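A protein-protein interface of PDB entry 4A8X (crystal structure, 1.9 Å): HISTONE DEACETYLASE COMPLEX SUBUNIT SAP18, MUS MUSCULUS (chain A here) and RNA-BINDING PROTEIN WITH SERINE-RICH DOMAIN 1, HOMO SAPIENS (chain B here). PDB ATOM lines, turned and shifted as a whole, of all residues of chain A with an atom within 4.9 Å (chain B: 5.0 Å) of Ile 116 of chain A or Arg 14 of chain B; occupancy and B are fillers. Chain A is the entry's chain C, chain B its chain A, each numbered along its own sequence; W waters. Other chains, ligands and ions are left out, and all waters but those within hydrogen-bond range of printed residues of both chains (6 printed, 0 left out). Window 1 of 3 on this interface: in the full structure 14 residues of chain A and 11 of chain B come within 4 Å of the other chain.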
ATOM      1  N   LEU A  15       5.310  22.918 -28.178  1.00  0.00           N
ATOM      2  CA  LEU A  15       6.015  21.724 -28.606  1.00  0.00           C
ATOM      3  C   LEU A  15       5.056  20.907 -29.426  1.00  0.00           C
ATOM      4  O   LEU A  15       3.825  20.994 -29.222  1.00  0.00           O
ATOM      5  CB  LEU A  15       6.482  20.902 -27.369  1.00  0.00           C
ATOM      6  CG  LEU A  15       5.387  20.361 -26.443  1.00  0.00           C
ATOM      7  CD1 LEU A  15       5.129  18.874 -26.643  1.00  0.00           C
ATOM      8  CD2 LEU A  15       5.681  20.670 -24.959  1.00  0.00           C
ATOM      9  N   LEU A  16       5.613  20.141 -30.365  1.00  0.00           N
ATOM     10  CA  LEU A  16       4.839  19.209 -31.170  1.00  0.00           C
ATOM     11  C   LEU A  16       4.666  17.917 -30.361  1.00  0.00           C
ATOM     12  O   LEU A  16       5.652  17.298 -29.962  1.00  0.00           O
ATOM     13  CB  LEU A  16       5.572  18.837 -32.451  1.00  0.00           C
ATOM     14  CG  LEU A  16       4.946  17.672 -33.254  1.00  0.00           C
ATOM     15  CD1 LEU A  16       3.584  18.025 -33.779  1.00  0.00           C
ATOM     16  CD2 LEU A  16       5.879  17.283 -34.400  1.00  0.00           C
ATOM     17  N   MET A  49       4.519  22.304 -21.741  1.00  0.00           N
ATOM     18  CA  MET A  49       5.011  21.315 -20.795  1.00  0.00           C
ATOM     19  C   MET A  49       4.077  21.223 -19.571  1.00  0.00           C
ATOM     20  O   MET A  49       4.115  20.228 -18.842  1.00  0.00           O
ATOM     21  CB  MET A  49       6.436  21.677 -20.363  1.00  0.00           C
ATOM     22  CG  MET A  49       7.533  21.262 -21.388  1.00  0.00           C
ATOM     23  SD  MET A  49       7.469  19.506 -21.848  1.00  0.00           S
ATOM     24  CE  MET A  49       7.961  18.805 -20.264  1.00  0.00           C
ATOM     25  N   MET A  81      11.883   6.410 -25.919  1.00  0.00           N
ATOM     26  CA  MET A  81      13.068   5.630 -26.204  1.00  0.00           C
ATOM     27  C   MET A  81      13.913   5.624 -24.948  1.00  0.00           C
ATOM     28  O   MET A  81      14.146   6.658 -24.326  1.00  0.00           O
ATOM     29  CB  MET A  81      13.852   6.206 -27.397  1.00  0.00           C
ATOM     30  CG  MET A  81      15.232   5.564 -27.620  1.00  0.00           C
ATOM     31  SD  MET A  81      15.268   3.755 -27.903  1.00  0.00           S
ATOM     32  CE  MET A  81      14.456   3.632 -29.501  1.00  0.00           C
ATOM     33  N   PHE A 114       8.111  13.888 -18.752  1.00  0.00           N
ATOM     34  CA  PHE A 114       7.943  13.801 -20.181  1.00  0.00           C
ATOM     35  C   PHE A 114       9.070  14.587 -20.865  1.00  0.00           C
ATOM     36  O   PHE A 114       9.392  15.704 -20.463  1.00  0.00           O
ATOM     37  CB  PHE A 114       6.586  14.411 -20.544  1.00  0.00           C
ATOM     38  CG  PHE A 114       6.351  14.547 -22.033  1.00  0.00           C
ATOM     39  CD1 PHE A 114       5.773  13.516 -22.742  1.00  0.00           C
ATOM     40  CD2 PHE A 114       6.689  15.706 -22.705  1.00  0.00           C
ATOM     41  CE1 PHE A 114       5.570  13.626 -24.128  1.00  0.00           C
ATOM     42  CE2 PHE A 114       6.478  15.812 -24.064  1.00  0.00           C
ATOM     43  CZ  PHE A 114       5.910  14.776 -24.765  1.00  0.00           C
ATOM     44  N   GLN A 115       9.673  14.004 -21.893  1.00  0.00           N
ATOM     45  CA  GLN A 115      10.665  14.730 -22.692  1.00  0.00           C
ATOM     46  C   GLN A 115      10.103  14.937 -24.071  1.00  0.00           C
ATOM     47  O   GLN A 115       9.545  14.008 -24.658  1.00  0.00           O
ATOM     48  CB  GLN A 115      11.959  13.943 -22.802  1.00  0.00           C
ATOM     49  CG  GLN A 115      12.651  13.716 -21.467  1.00  0.00           C
ATOM     50  CD  GLN A 115      13.928  12.935 -21.620  1.00  0.00           C
ATOM     51  OE1 GLN A 115      14.606  13.027 -22.643  1.00  0.00           O
ATOM     52  NE2 GLN A 115      14.264  12.142 -20.605  1.00  0.00           N
ATOM     53  N   ILE A 116      10.273  16.148 -24.601  1.00  0.00           N
ATOM     54  CA  ILE A 116       9.689  16.489 -25.885  1.00  0.00           C
ATOM     55  C   ILE A 116      10.163  15.538 -26.983  1.00  0.00           C
ATOM     56  O   ILE A 116      11.346  15.260 -27.107  1.00  0.00           O
ATOM     57  CB  ILE A 116      10.027  17.971 -26.252  1.00  0.00           C
ATOM     58  CG1 ILE A 116       9.343  18.918 -25.256  1.00  0.00           C
ATOM     59  CG2 ILE A 116       9.584  18.261 -27.656  1.00  0.00           C
ATOM     60  CD1 ILE A 116       9.802  20.367 -25.364  1.00  0.00           C
ATOM     61  N   GLY A 117       9.222  15.015 -27.750  1.00  0.00           N
ATOM     62  CA  GLY A 117       9.549  13.991 -28.715  1.00  0.00           C
ATOM     63  C   GLY A 117       9.054  12.622 -28.282  1.00  0.00           C
ATOM     64  O   GLY A 117       8.889  11.745 -29.118  1.00  0.00           O
ATOM     65  N   ASP A 118       8.866  12.434 -26.980  1.00  0.00           N
ATOM     66  CA  ASP A 118       8.256  11.197 -26.481  1.00  0.00           C
ATOM     67  C   ASP A 118       6.848  11.149 -27.061  1.00  0.00           C
ATOM     68  O   ASP A 118       6.179  12.197 -27.176  1.00  0.00           O
ATOM     69  CB  ASP A 118       8.146  11.210 -24.951  1.00  0.00           C
ATOM     70  CG  ASP A 118       9.485  11.082 -24.235  1.00  0.00           C
ATOM     71  OD1 ASP A 118      10.487  10.683 -24.864  1.00  0.00           O
ATOM     72  OD2 ASP A 118       9.506  11.335 -22.996  1.00  0.00           O
ATOM     73  N   LEU B  12      18.399  20.334 -28.786  1.00  0.00           N
ATOM     74  CA  LEU B  12      17.416  20.100 -29.822  1.00  0.00           C
ATOM     75  C   LEU B  12      16.513  18.975 -29.352  1.00  0.00           C
ATOM     76  O   LEU B  12      17.024  17.925 -28.917  1.00  0.00           O
ATOM     77  CB  LEU B  12      18.117  19.702 -31.130  1.00  0.00           C
ATOM     78  CG  LEU B  12      18.997  20.776 -31.797  1.00  0.00           C
ATOM     79  CD1 LEU B  12      19.639  20.294 -33.128  1.00  0.00           C
ATOM     80  CD2 LEU B  12      18.174  22.055 -32.072  1.00  0.00           C
ATOM     81  N   THR B  13      15.193  19.156 -29.427  1.00  0.00           N
ATOM     82  CA  THR B  13      14.300  18.054 -29.112  1.00  0.00           C
ATOM     83  C   THR B  13      14.427  16.887 -30.090  1.00  0.00           C
ATOM     84  O   THR B  13      14.979  17.032 -31.195  1.00  0.00           O
ATOM     85  CB  THR B  13      12.828  18.461 -29.017  1.00  0.00           C
ATOM     86  OG1 THR B  13      12.284  18.542 -30.314  1.00  0.00           O
ATOM     87  CG2 THR B  13      12.652  19.775 -28.263  1.00  0.00           C
ATOM     88  N   ARG B  14      13.897  15.724 -29.673  1.00  0.00           N
ATOM     89  CA  ARG B  14      13.856  14.543 -30.520  1.00  0.00           C
ATOM     90  C   ARG B  14      12.952  14.686 -31.761  1.00  0.00           C
ATOM     91  O   ARG B  14      12.974  13.848 -32.649  1.00  0.00           O
ATOM     92  CB  ARG B  14      13.444  13.347 -29.641  1.00  0.00           C
ATOM     93  CG  ARG B  14      13.345  11.988 -30.302  1.00  0.00           C
ATOM     94  CD  ARG B  14      13.504  10.918 -29.199  1.00  0.00           C
ATOM     95  NE  ARG B  14      14.877  10.906 -28.693  1.00  0.00           N
ATOM     96  CZ  ARG B  14      15.261  10.328 -27.561  1.00  0.00           C
ATOM     97  NH1 ARG B  14      14.380   9.710 -26.771  1.00  0.00           N
ATOM     98  NH2 ARG B  14      16.536  10.368 -27.213  1.00  0.00           N
ATOM     99  N   ASN B  15      12.119  15.729 -31.827  1.00  0.00           N
ATOM    100  CA  ASN B  15      11.352  15.990 -33.046  1.00  0.00           C
ATOM    101  C   ASN B  15      12.187  16.723 -34.134  1.00  0.00           C
ATOM    102  O   ASN B  15      11.787  16.762 -35.300  1.00  0.00           O
ATOM    103  CB  ASN B  15      10.130  16.907 -32.763  1.00  0.00           C
ATOM    104  CG  ASN B  15       9.027  16.228 -32.012  1.00  0.00           C
ATOM    105  OD1 ASN B  15       8.729  15.044 -32.217  1.00  0.00           O
ATOM    106  ND2 ASN B  15       8.384  16.979 -31.130  1.00  0.00           N
ATOM    107  N   VAL B  16      13.300  17.357 -33.757  1.00  0.00           N
ATOM    108  CA  VAL B  16      14.000  18.259 -34.709  1.00  0.00           C
ATOM    109  C   VAL B  16      14.840  17.479 -35.728  1.00  0.00           C
ATOM    110  O   VAL B  16      15.696  16.681 -35.345  1.00  0.00           O
ATOM    111  CB  VAL B  16      14.899  19.294 -33.948  1.00  0.00           C
ATOM    112  CG1 VAL B  16      15.670  20.192 -34.939  1.00  0.00           C
ATOM    113  CG2 VAL B  16      14.053  20.143 -32.996  1.00  0.00           C
ATOM    114  N   LEU B  45      17.164   8.577 -34.738  1.00  0.00           N
ATOM    115  CA  LEU B  45      17.155   9.591 -33.704  1.00  0.00           C
ATOM    116  C   LEU B  45      18.463  10.365 -33.692  1.00  0.00           C
ATOM    117  O   LEU B  45      19.532   9.797 -33.865  1.00  0.00           O
ATOM    118  CB  LEU B  45      16.964   8.956 -32.327  1.00  0.00           C
ATOM    119  CG  LEU B  45      15.659   8.170 -32.119  1.00  0.00           C
ATOM    120  CD1 LEU B  45      15.629   7.618 -30.725  1.00  0.00           C
ATOM    121  CD2 LEU B  45      14.463   9.075 -32.357  1.00  0.00           C
ATOM    122  N   ASP B  73      11.041  23.952 -31.377  1.00  0.00           N
ATOM    123  CA  ASP B  73      10.042  22.970 -30.945  1.00  0.00           C
ATOM    124  C   ASP B  73       9.740  23.022 -29.457  1.00  0.00           C
ATOM    125  O   ASP B  73       9.764  21.977 -28.776  1.00  0.00           O
ATOM    126  CB  ASP B  73      10.482  21.543 -31.323  1.00  0.00           C
ATOM    127  CG  ASP B  73       9.388  20.527 -31.115  1.00  0.00           C
ATOM    128  OD1 ASP B  73       8.191  20.873 -31.273  1.00  0.00           O
ATOM    129  OD2 ASP B  73       9.738  19.364 -30.777  1.00  0.00           O
ATOM    130  N   GLY B  74       9.504  24.231 -28.941  1.00  0.00           N
ATOM    131  CA  GLY B  74       9.010  24.425 -27.594  1.00  0.00           C
ATOM    132  C   GLY B  74      10.065  24.333 -26.523  1.00  0.00           C
ATOM    133  O   GLY B  74       9.750  24.287 -25.343  1.00  0.00           O
ATOM    134  N   GLN B  75      11.322  24.295 -26.935  1.00  0.00           N
ATOM    135  CA  GLN B  75      12.427  24.150 -26.013  1.00  0.00           C
ATOM    136  C   GLN B  75      13.499  25.217 -26.281  1.00  0.00           C
ATOM    137  O   GLN B  75      13.856  25.502 -27.428  1.00  0.00           O
ATOM    138  CB  GLN B  75      13.039  22.736 -26.148  1.00  0.00           C
ATOM    139  CG  GLN B  75      14.102  22.422 -25.112  1.00  0.00           C
ATOM    140  CD  GLN B  75      14.237  20.935 -24.907  1.00  0.00           C
ATOM    141  OE1 GLN B  75      13.411  20.311 -24.220  1.00  0.00           O
ATOM    142  NE2 GLN B  75      15.249  20.337 -25.555  1.00  0.00           N
HETATM  143  O   HOH W   1       7.231  12.915 -31.129  1.00  0.00           O
HETATM  144  O   HOH W   2      12.433  17.938 -23.329  1.00  0.00           O
HETATM  145  O   HOH W   3      13.860  15.939 -26.382  1.00  0.00           O
HETATM  146  O   HOH W   4       6.816  22.854 -32.059  1.00  0.00           O
HETATM  147  O   HOH W   5      12.225  12.431 -26.391  1.00  0.00           O
HETATM  148  O   HOH W   6      11.591   9.133 -26.759  1.00  0.00           O
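Printed residues of chain B that touch a printed residue of chain A: Thr 13, Arg 14, Asn 15, Leu 45, Asp 73, Gly 74 and Gln 75. Among the printed residues, no Asp or Glu carboxylate lies within 4 Å of a Lys or Arg side-chain nitrogen of the other chain.
Arg 14 of chain B touches just these residues of chain A: Met 81 and Ile 116. Of the printed residues of chain A, Thr 13 of chain B touches Ile 116. Of the printed residues of chain B, Leu 15 of chain A touches Asp 73. Asp 118 of chain A touches none of the printed residues of chain B. The nearest printed residue of chain B that does not touch Ile 116 of chain A is Leu 12 of chain B (6.5 Å).
Water W4 lies within hydrogen-bond range of the side-chain carboxylate (OD1) of Asp 73 of chain B and the backbone NH (N) of Leu 16 of chain A. Water W6 lies within hydrogen-bond range of OD1 of Asp 118 of chain A (2.7 Å), NH1 of Arg 14 of chain B (2.8 Å) and N of Met 81 of chain A (2.9 Å). Water W3 lies within hydrogen-bond range of the backbone carbonyl oxygen of Ile 116 of chain A and the backbone NH of Arg 14 of chain B. Water W2 bridges the side-chain amide oxygen of Gln 75 of chain B and the backbone NH of Ile 116 of chain A. Water W1 lies within hydrogen-bond range of OD1 of Asn 15 of chain B and O of Gly 117 of chain A. Water W5 lies within hydrogen-bond range of the side-chain carboxylate of Asp 118 of chain A, the backbone carbonyl oxygen of Ile 116 of chain A and the guanidinium group of Arg 14 of chain B.
O of Leu 16 of chain A is in hydrogen-bond range of ND2 of Asn 15 of chain B, at 3.0 Å. N of Leu 16 of chain A sits at hydrogen-bond distance from OD1 of Asp 73 of chain B (2.8 Å).
The side-chain hydroxyl (OG1) of Thr 13 of chain B lies close to the backbone NH (N) of Asn 15 of chain B (3.2 Å). The side-chain hydroxyl (OG1) of Thr 13 of chain B sits at hydrogen-bond distance from the side-chain carboxylate (OD2) of Asp 73 of chain B. The side-chain amide nitrogen of Asn 15 of chain B is in hydrogen-bond range of the side-chain carboxylate of Asp 73 of chain B (2.8 Å).
Among the printed residues, pairs that only touch across the chains: Ile 116 of chain A with Asp 73 of chain B, Ile 116 of chain A with Thr 13 of chain B, Leu 15 of chain A with Asp 73 of chain B, Met 81 of chain A with Arg 14 of chain B, Ile 116 of chain A with Arg 14 of chain B, Met 81 of chain A with Leu 45 of chain B, Gly 117 of chain A with Asn 15 of chain B, Ile 116 of chain A with Gln 75 of chain B, Ile 116 of chain A with Asn 15 of chain B and Ile 116 of chain A with Gly 74 of chain B.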
